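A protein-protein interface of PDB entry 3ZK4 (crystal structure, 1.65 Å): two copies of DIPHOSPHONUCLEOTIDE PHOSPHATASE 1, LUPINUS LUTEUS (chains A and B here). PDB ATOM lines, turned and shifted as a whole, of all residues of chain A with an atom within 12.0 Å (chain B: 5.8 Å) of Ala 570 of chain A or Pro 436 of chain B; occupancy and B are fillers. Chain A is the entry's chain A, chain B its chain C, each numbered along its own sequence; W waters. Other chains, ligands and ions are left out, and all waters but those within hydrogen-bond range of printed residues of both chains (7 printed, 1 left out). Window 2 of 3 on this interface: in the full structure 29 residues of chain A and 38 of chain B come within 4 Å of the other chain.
N of Thr 568 of chain A is in hydrogen-bond range of O of Phe 338 of chain B, at 2.9 Å. The chain-end carboxylate of Ser 571 of chain A lies within hydrogen-bond range of the side-chain amide nitrogen of Asn 341 of chain B (2.9 Å).
The side-chain hydroxyl of Thr 568 of chain A lies within hydrogen-bond range of the backbone NH of Ala 570 of chain A. OE2 of Glu 435 of chain B sits at hydrogen-bond distance from OH of Tyr 427 of chain B, at 2.7 Å. The side-chain hydroxyl (OH) of Tyr 339 of chain B sits at hydrogen-bond distance from the side-chain carboxylate (OE1) of Glu 435 of chain B. The backbone carbonyl oxygen (O) of Met 437 of chain B is in hydrogen-bond range of the indole nitrogen (NE1) of Trp 386 of chain B (3.0 Å).
Among the printed residues, pairs that only touch across the chains: Thr 566 of chain A with Phe 338 of chain B, Thr 567 of chain A with Phe 338 of chain B, Thr 568 of chain A with Tyr 339 of chain B, Thr 568 of chain A with Met 437 of chain B, Ala 570 of chain A with Tyr 339 of chain B, Ala 570 of chain A with Pro 436 of chain B and Ser 571 of chain A with Glu 435 of chain B.
Ala 570 of chain A touches two residues of chain B. Pro 436 of chain B touches just one residue of chain A: Ala 570 (3.7 Å). Tyr 339 of chain B touches just these residues of chain A: Thr 568 (3.6 Å) and Ala 570 (3.3 Å). No residue of chain A comes within 4 Å of Gly 340 of chain B. No residue of chain A comes within 4 Å of Ser 432 of chain B. No residue of chain A comes within 4 Å of Gly 438 of chain B. Printed residues of chain A within 4 Å of Asn 341 of chain B: Ser 571 (2.9 Å). Printed residues of chain B within 4 Å of Thr 568 of chain A: Phe 338, Tyr 339 and Met 437. Of the printed residues of chain B, Ser 571 of chain A touches Asn 341 and Glu 435. Of the printed residues of chain B, Thr 567 of chain A touches Phe 338 (3.4 Å). Glu 440 of chain B touches none of the printed residues of chain A. Glu 430 of chain B touches none of the printed residues of chain A. The nearest printed residue of chain B that does not touch Thr 567 of chain A is Met 437 of chain B (5.4 Å).
Printed residues of chain B that touch a printed residue of chain A: Phe 338, Tyr 339, Asn 341, Glu 435, Pro 436 and Met 437. Hydrophobic or aromatic side chains of chain B that line the printed part of chain A: Phe 338, Tyr 339, Pro 436 and Met 437. Among the printed residues, 9 pairs touch across the chains.
No position is printed for both chains. Of the 9 pairs that touch across the chains among the printed residues, none has its exchanged pair printed and touching as well.
Water W2 lies within hydrogen-bond range of the side-chain carboxylate of Glu 430 of chain B (2.7 Å) and the backbone NH of Ser 571 of chain A (2.8 Å). Water W1 lies within hydrogen-bond range of OD1 of Asn 341 of chain B (2.8 Å) and OG of Ser 571 of chain A (2.9 Å). Water W5 lies within hydrogen-bond range of OXT of Ser 571 of chain A (2.8 Å) and OE2 of Glu 435 of chain B (2.9 Å). Water W7 lies within hydrogen-bond range of OG1 of Thr 568 of chain A, O of Pro 436 of chain B and OH of Tyr 339 of chain B. Water W4 lies within hydrogen-bond range of O of Thr 568 of chain A (2.8 Å) and N of Gly 340 of chain B (3.5 Å). Water W3 lies within hydrogen-bond range of O of Thr 566 of chain A (3.1 Å) and N of Phe 338 of chain B (3.3 Å).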
ATOM      1  N   THR A 566       1.849  -9.806 -28.751  1.00  0.00           N
ATOM      2  CA  THR A 566       2.812 -10.788 -28.284  1.00  0.00           C
ATOM      3  C   THR A 566       3.202 -11.748 -29.368  1.00  0.00           C
ATOM      4  O   THR A 566       2.454 -11.978 -30.319  1.00  0.00           O
ATOM      5  CB  THR A 566       2.247 -11.670 -27.133  1.00  0.00           C
ATOM      6  OG1 THR A 566       0.970 -12.271 -27.512  1.00  0.00           O
ATOM      7  CG2 THR A 566       2.097 -10.852 -25.941  1.00  0.00           C
ATOM      8  N   THR A 567       4.383 -12.341 -29.199  1.00  0.00           N
ATOM      9  CA  THR A 567       4.832 -13.374 -30.114  1.00  0.00           C
ATOM     10  C   THR A 567       5.422 -14.555 -29.381  1.00  0.00           C
ATOM     11  O   THR A 567       5.726 -14.490 -28.201  1.00  0.00           O
ATOM     12  CB  THR A 567       5.907 -12.869 -31.071  1.00  0.00           C
ATOM     13  OG1 THR A 567       6.925 -12.249 -30.305  1.00  0.00           O
ATOM     14  CG2 THR A 567       5.337 -11.899 -32.047  1.00  0.00           C
ATOM     15  N   THR A 568       5.538 -15.648 -30.096  1.00  0.00           N
ATOM     16  CA  THR A 568       6.334 -16.782 -29.626  1.00  0.00           C
ATOM     17  C   THR A 568       7.584 -16.885 -30.509  1.00  0.00           C
ATOM     18  O   THR A 568       7.525 -16.515 -31.696  1.00  0.00           O
ATOM     19  CB  THR A 568       5.536 -18.101 -29.634  1.00  0.00           C
ATOM     20  OG1 THR A 568       6.395 -19.183 -29.209  1.00  0.00           O
ATOM     21  CG2 THR A 568       4.978 -18.484 -31.000  1.00  0.00           C
ATOM     22  N   LEU A 569       8.704 -17.334 -29.919  1.00  0.00           N
ATOM     23  CA  LEU A 569       9.888 -17.640 -30.694  1.00  0.00           C
ATOM     24  C   LEU A 569       9.779 -18.917 -31.480  1.00  0.00           C
ATOM     25  O   LEU A 569      10.570 -19.089 -32.439  1.00  0.00           O
ATOM     26  CB  LEU A 569      11.119 -17.724 -29.835  1.00  0.00           C
ATOM     27  CG  LEU A 569      11.551 -16.415 -29.186  1.00  0.00           C
ATOM     28  CD1 LEU A 569      12.847 -16.634 -28.424  1.00  0.00           C
ATOM     29  CD2 LEU A 569      11.699 -15.328 -30.251  1.00  0.00           C
ATOM     30  N   ALA A 570       8.800 -19.765 -31.153  1.00  0.00           N
ATOM     31  CA  ALA A 570       8.643 -21.090 -31.760  1.00  0.00           C
ATOM     32  C   ALA A 570       8.116 -20.994 -33.200  1.00  0.00           C
ATOM     33  O   ALA A 570       7.602 -19.933 -33.596  1.00  0.00           O
ATOM     34  CB  ALA A 570       7.754 -21.967 -30.900  1.00  0.00           C
ATOM     35  N   SER A 571       8.292 -22.079 -33.955  1.00  0.00           N
ATOM     36  CA  SER A 571       7.829 -22.215 -35.359  1.00  0.00           C
ATOM     37  C   SER A 571       6.873 -23.364 -35.496  1.00  0.00           C
ATOM     38  O   SER A 571       6.032 -23.428 -36.439  1.00  0.00           O
ATOM     39  CB  SER A 571       8.996 -22.456 -36.299  1.00  0.00           C
ATOM     40  OG  SER A 571       9.890 -21.371 -36.287  1.00  0.00           O
ATOM     41  OXT SER A 571       6.948 -24.333 -34.697  1.00  0.00           O
ATOM     42  N   PHE B 338       0.927 -14.649 -33.820  1.00  0.00           N
ATOM     43  CA  PHE B 338       1.693 -15.046 -32.645  1.00  0.00           C
ATOM     44  C   PHE B 338       2.959 -15.789 -33.112  1.00  0.00           C
ATOM     45  O   PHE B 338       4.042 -15.526 -32.608  1.00  0.00           O
ATOM     46  CB  PHE B 338       0.778 -15.929 -31.801  1.00  0.00           C
ATOM     47  CG  PHE B 338       1.338 -16.299 -30.426  1.00  0.00           C
ATOM     48  CD1 PHE B 338       1.804 -15.351 -29.556  1.00  0.00           C
ATOM     49  CD2 PHE B 338       1.349 -17.620 -30.018  1.00  0.00           C
ATOM     50  CE1 PHE B 338       2.289 -15.720 -28.294  1.00  0.00           C
ATOM     51  CE2 PHE B 338       1.831 -18.006 -28.757  1.00  0.00           C
ATOM     52  CZ  PHE B 338       2.307 -17.052 -27.906  1.00  0.00           C
ATOM     53  N   TYR B 339       2.787 -16.605 -34.168  1.00  0.00           N
ATOM     54  CA  TYR B 339       3.891 -17.242 -34.945  1.00  0.00           C
ATOM     55  C   TYR B 339       4.264 -16.352 -36.123  1.00  0.00           C
ATOM     56  O   TYR B 339       3.361 -15.907 -36.867  1.00  0.00           O
ATOM     57  CB  TYR B 339       3.440 -18.607 -35.440  1.00  0.00           C
ATOM     58  CG  TYR B 339       3.348 -19.629 -34.328  1.00  0.00           C
ATOM     59  CD1 TYR B 339       2.214 -19.727 -33.506  1.00  0.00           C
ATOM     60  CD2 TYR B 339       4.407 -20.493 -34.075  1.00  0.00           C
ATOM     61  CE1 TYR B 339       2.158 -20.634 -32.450  1.00  0.00           C
ATOM     62  CE2 TYR B 339       4.353 -21.398 -33.044  1.00  0.00           C
ATOM     63  CZ  TYR B 339       3.230 -21.472 -32.227  1.00  0.00           C
ATOM     64  OH  TYR B 339       3.206 -22.381 -31.205  1.00  0.00           O
ATOM     65  N   GLY B 340       5.561 -16.107 -36.268  1.00  0.00           N
ATOM     66  CA  GLY B 340       6.085 -15.246 -37.310  1.00  0.00           C
ATOM     67  C   GLY B 340       6.546 -15.979 -38.559  1.00  0.00           C
ATOM     68  O   GLY B 340       7.241 -15.366 -39.385  1.00  0.00           O
ATOM     69  N   ASN B 341       6.146 -17.230 -38.713  1.00  0.00           N
ATOM     70  CA  ASN B 341       6.529 -18.071 -39.867  1.00  0.00           C
ATOM     71  C   ASN B 341       6.071 -17.413 -41.172  1.00  0.00           C
ATOM     72  O   ASN B 341       5.140 -16.595 -41.179  1.00  0.00           O
ATOM     73  CB  ASN B 341       5.845 -19.440 -39.828  1.00  0.00           C
ATOM     74  CG  ASN B 341       6.158 -20.250 -38.572  1.00  0.00           C
ATOM     75  OD1 ASN B 341       6.538 -19.701 -37.517  1.00  0.00           O
ATOM     76  ND2 ASN B 341       5.981 -21.557 -38.669  1.00  0.00           N
ATOM     77  N   TRP B 386      -3.035 -17.581 -27.023  1.00  0.00           N
ATOM     78  CA  TRP B 386      -4.100 -18.266 -26.333  1.00  0.00           C
ATOM     79  C   TRP B 386      -3.924 -18.294 -24.810  1.00  0.00           C
ATOM     80  O   TRP B 386      -4.716 -18.933 -24.101  1.00  0.00           O
ATOM     81  CB  TRP B 386      -4.175 -19.713 -26.791  1.00  0.00           C
ATOM     82  CG  TRP B 386      -2.853 -20.415 -26.600  1.00  0.00           C
ATOM     83  CD1 TRP B 386      -2.394 -20.910 -25.438  1.00  0.00           C
ATOM     84  CD2 TRP B 386      -1.834 -20.670 -27.582  1.00  0.00           C
ATOM     85  NE1 TRP B 386      -1.149 -21.499 -25.619  1.00  0.00           N
ATOM     86  CE2 TRP B 386      -0.779 -21.341 -26.921  1.00  0.00           C
ATOM     87  CE3 TRP B 386      -1.716 -20.424 -28.955  1.00  0.00           C
ATOM     88  CZ2 TRP B 386       0.391 -21.746 -27.562  1.00  0.00           C
ATOM     89  CZ3 TRP B 386      -0.554 -20.837 -29.600  1.00  0.00           C
ATOM     90  CH2 TRP B 386       0.487 -21.465 -28.922  1.00  0.00           C
ATOM     91  N   TYR B 427       8.453 -31.606 -32.665  1.00  0.00           N
ATOM     92  CA  TYR B 427       8.283 -31.097 -31.305  1.00  0.00           C
ATOM     93  C   TYR B 427       9.369 -31.654 -30.391  1.00  0.00           C
ATOM     94  O   TYR B 427       9.992 -30.934 -29.604  1.00  0.00           O
ATOM     95  CB  TYR B 427       6.916 -31.459 -30.740  1.00  0.00           C
ATOM     96  CG  TYR B 427       5.730 -30.692 -31.336  1.00  0.00           C
ATOM     97  CD1 TYR B 427       5.799 -29.318 -31.520  1.00  0.00           C
ATOM     98  CD2 TYR B 427       4.520 -31.332 -31.596  1.00  0.00           C
ATOM     99  CE1 TYR B 427       4.719 -28.603 -32.064  1.00  0.00           C
ATOM    100  CE2 TYR B 427       3.454 -30.635 -32.111  1.00  0.00           C
ATOM    101  CZ  TYR B 427       3.551 -29.274 -32.324  1.00  0.00           C
ATOM    102  OH  TYR B 427       2.417 -28.615 -32.827  1.00  0.00           O
ATOM    103  N   GLU B 430      12.749 -30.006 -30.327  1.00  0.00           N
ATOM    104  CA  GLU B 430      12.882 -28.755 -29.608  1.00  0.00           C
ATOM    105  C   GLU B 430      12.568 -28.935 -28.118  1.00  0.00           C
ATOM    106  O   GLU B 430      12.409 -27.959 -27.388  1.00  0.00           O
ATOM    107  CB  GLU B 430      12.045 -27.633 -30.240  1.00  0.00           C
ATOM    108  CG  GLU B 430      10.550 -27.873 -30.202  1.00  0.00           C
ATOM    109  CD  GLU B 430       9.707 -26.712 -30.742  1.00  0.00           C
ATOM    110  OE1 GLU B 430      10.255 -25.589 -30.903  1.00  0.00           O
ATOM    111  OE2 GLU B 430       8.486 -26.942 -30.980  1.00  0.00           O
ATOM    112  N   SER B 432       9.956 -30.693 -26.611  1.00  0.00           N
ATOM    113  CA  SER B 432       8.538 -30.506 -26.276  1.00  0.00           C
ATOM    114  C   SER B 432       7.694 -31.636 -26.852  1.00  0.00           C
ATOM    115  O   SER B 432       8.116 -32.286 -27.828  1.00  0.00           O
ATOM    116  CB  SER B 432       8.130 -29.131 -26.813  1.00  0.00           C
ATOM    117  OG  SER B 432       6.883 -28.720 -26.278  1.00  0.00           O
ATOM    118  N   GLU B 434       4.340 -30.760 -27.624  1.00  0.00           N
ATOM    119  CA  GLU B 434       3.295 -29.720 -27.833  1.00  0.00           C
ATOM    120  C   GLU B 434       3.979 -28.519 -28.425  1.00  0.00           C
ATOM    121  O   GLU B 434       5.190 -28.331 -28.297  1.00  0.00           O
ATOM    122  CB  GLU B 434       2.682 -29.286 -26.483  1.00  0.00           C
ATOM    123  CG  GLU B 434       3.716 -28.835 -25.471  1.00  0.00           C
ATOM    124  CD  GLU B 434       3.200 -28.133 -24.210  1.00  0.00           C
ATOM    125  OE1 GLU B 434       2.000 -27.940 -24.097  1.00  0.00           O
ATOM    126  OE2 GLU B 434       4.017 -27.789 -23.308  1.00  0.00           O
ATOM    127  N   GLU B 435       3.202 -27.584 -28.968  1.00  0.00           N
ATOM    128  CA  GLU B 435       3.714 -26.239 -29.079  1.00  0.00           C
ATOM    129  C   GLU B 435       4.235 -25.752 -27.724  1.00  0.00           C
ATOM    130  O   GLU B 435       3.576 -25.960 -26.715  1.00  0.00           O
ATOM    131  CB  GLU B 435       2.621 -25.265 -29.515  1.00  0.00           C
ATOM    132  CG  GLU B 435       2.136 -25.465 -30.926  1.00  0.00           C
ATOM    133  CD  GLU B 435       3.219 -25.342 -31.987  1.00  0.00           C
ATOM    134  OE1 GLU B 435       4.266 -24.665 -31.823  1.00  0.00           O
ATOM    135  OE2 GLU B 435       3.033 -25.956 -33.054  1.00  0.00           O
ATOM    136  N   PRO B 436       5.371 -25.060 -27.708  1.00  0.00           N
ATOM    137  CA  PRO B 436       5.763 -24.357 -26.493  1.00  0.00           C
ATOM    138  C   PRO B 436       4.608 -23.544 -25.906  1.00  0.00           C
ATOM    139  O   PRO B 436       3.963 -22.801 -26.608  1.00  0.00           O
ATOM    140  CB  PRO B 436       6.960 -23.524 -26.946  1.00  0.00           C
ATOM    141  CG  PRO B 436       7.559 -24.350 -28.068  1.00  0.00           C
ATOM    142  CD  PRO B 436       6.348 -24.846 -28.784  1.00  0.00           C
ATOM    143  N   MET B 437       4.367 -23.717 -24.600  1.00  0.00           N
ATOM    144  CA  MET B 437       3.255 -23.019 -23.900  1.00  0.00           C
ATOM    145  C   MET B 437       1.857 -23.486 -24.306  1.00  0.00           C
ATOM    146  O   MET B 437       0.869 -22.868 -23.889  1.00  0.00           O
ATOM    147  CB  MET B 437       3.334 -21.495 -24.043  1.00  0.00           C
ATOM    148  CG  MET B 437       4.713 -20.955 -23.676  1.00  0.00           C
ATOM    149  SD  MET B 437       5.037 -19.245 -24.193  1.00  0.00           S
ATOM    150  CE  MET B 437       5.108 -19.424 -25.973  1.00  0.00           C
ATOM    151  N   GLY B 438       1.757 -24.581 -25.065  1.00  0.00           N
ATOM    152  CA  GLY B 438       0.457 -25.104 -25.528  1.00  0.00           C
ATOM    153  C   GLY B 438      -0.570 -25.348 -24.473  1.00  0.00           C
ATOM    154  O   GLY B 438      -1.692 -24.852 -24.571  1.00  0.00           O
ATOM    155  N   GLU B 440      -0.287 -25.356 -20.793  1.00  0.00           N
ATOM    156  CA  GLU B 440      -0.137 -25.083 -19.380  1.00  0.00           C
ATOM    157  C   GLU B 440      -1.238 -24.166 -18.847  1.00  0.00           C
ATOM    158  O   GLU B 440      -1.873 -24.489 -17.818  1.00  0.00           O
ATOM    159  CB  GLU B 440       1.280 -24.624 -19.104  1.00  0.00           C
ATOM    160  CG  GLU B 440       2.273 -25.798 -19.314  1.00  0.00           C
ATOM    161  CD  GLU B 440       2.664 -26.090 -20.788  1.00  0.00           C
ATOM    162  OE1 GLU B 440       2.396 -25.272 -21.691  1.00  0.00           O
ATOM    163  OE2 GLU B 440       3.295 -27.135 -21.057  1.00  0.00           O
HETATM  164  O   HOH W   1       9.057 -18.680 -37.098  1.00  0.00           O
HETATM  165  O   HOH W   2      10.188 -23.927 -32.971  1.00  0.00           O
HETATM  166  O   HOH W   3      -0.235 -12.455 -31.684  1.00  0.00           O
HETATM  167  O   HOH W   4       7.260 -14.528 -33.694  1.00  0.00           O
HETATM  168  O   HOH W   5       5.119 -26.427 -34.960  1.00  0.00           O
HETATM  169  O   HOH W   6       7.307 -17.446 -34.428  1.00  0.00           O
HETATM  170  O   HOH W   7       4.631 -21.342 -28.915  1.00  0.00           O
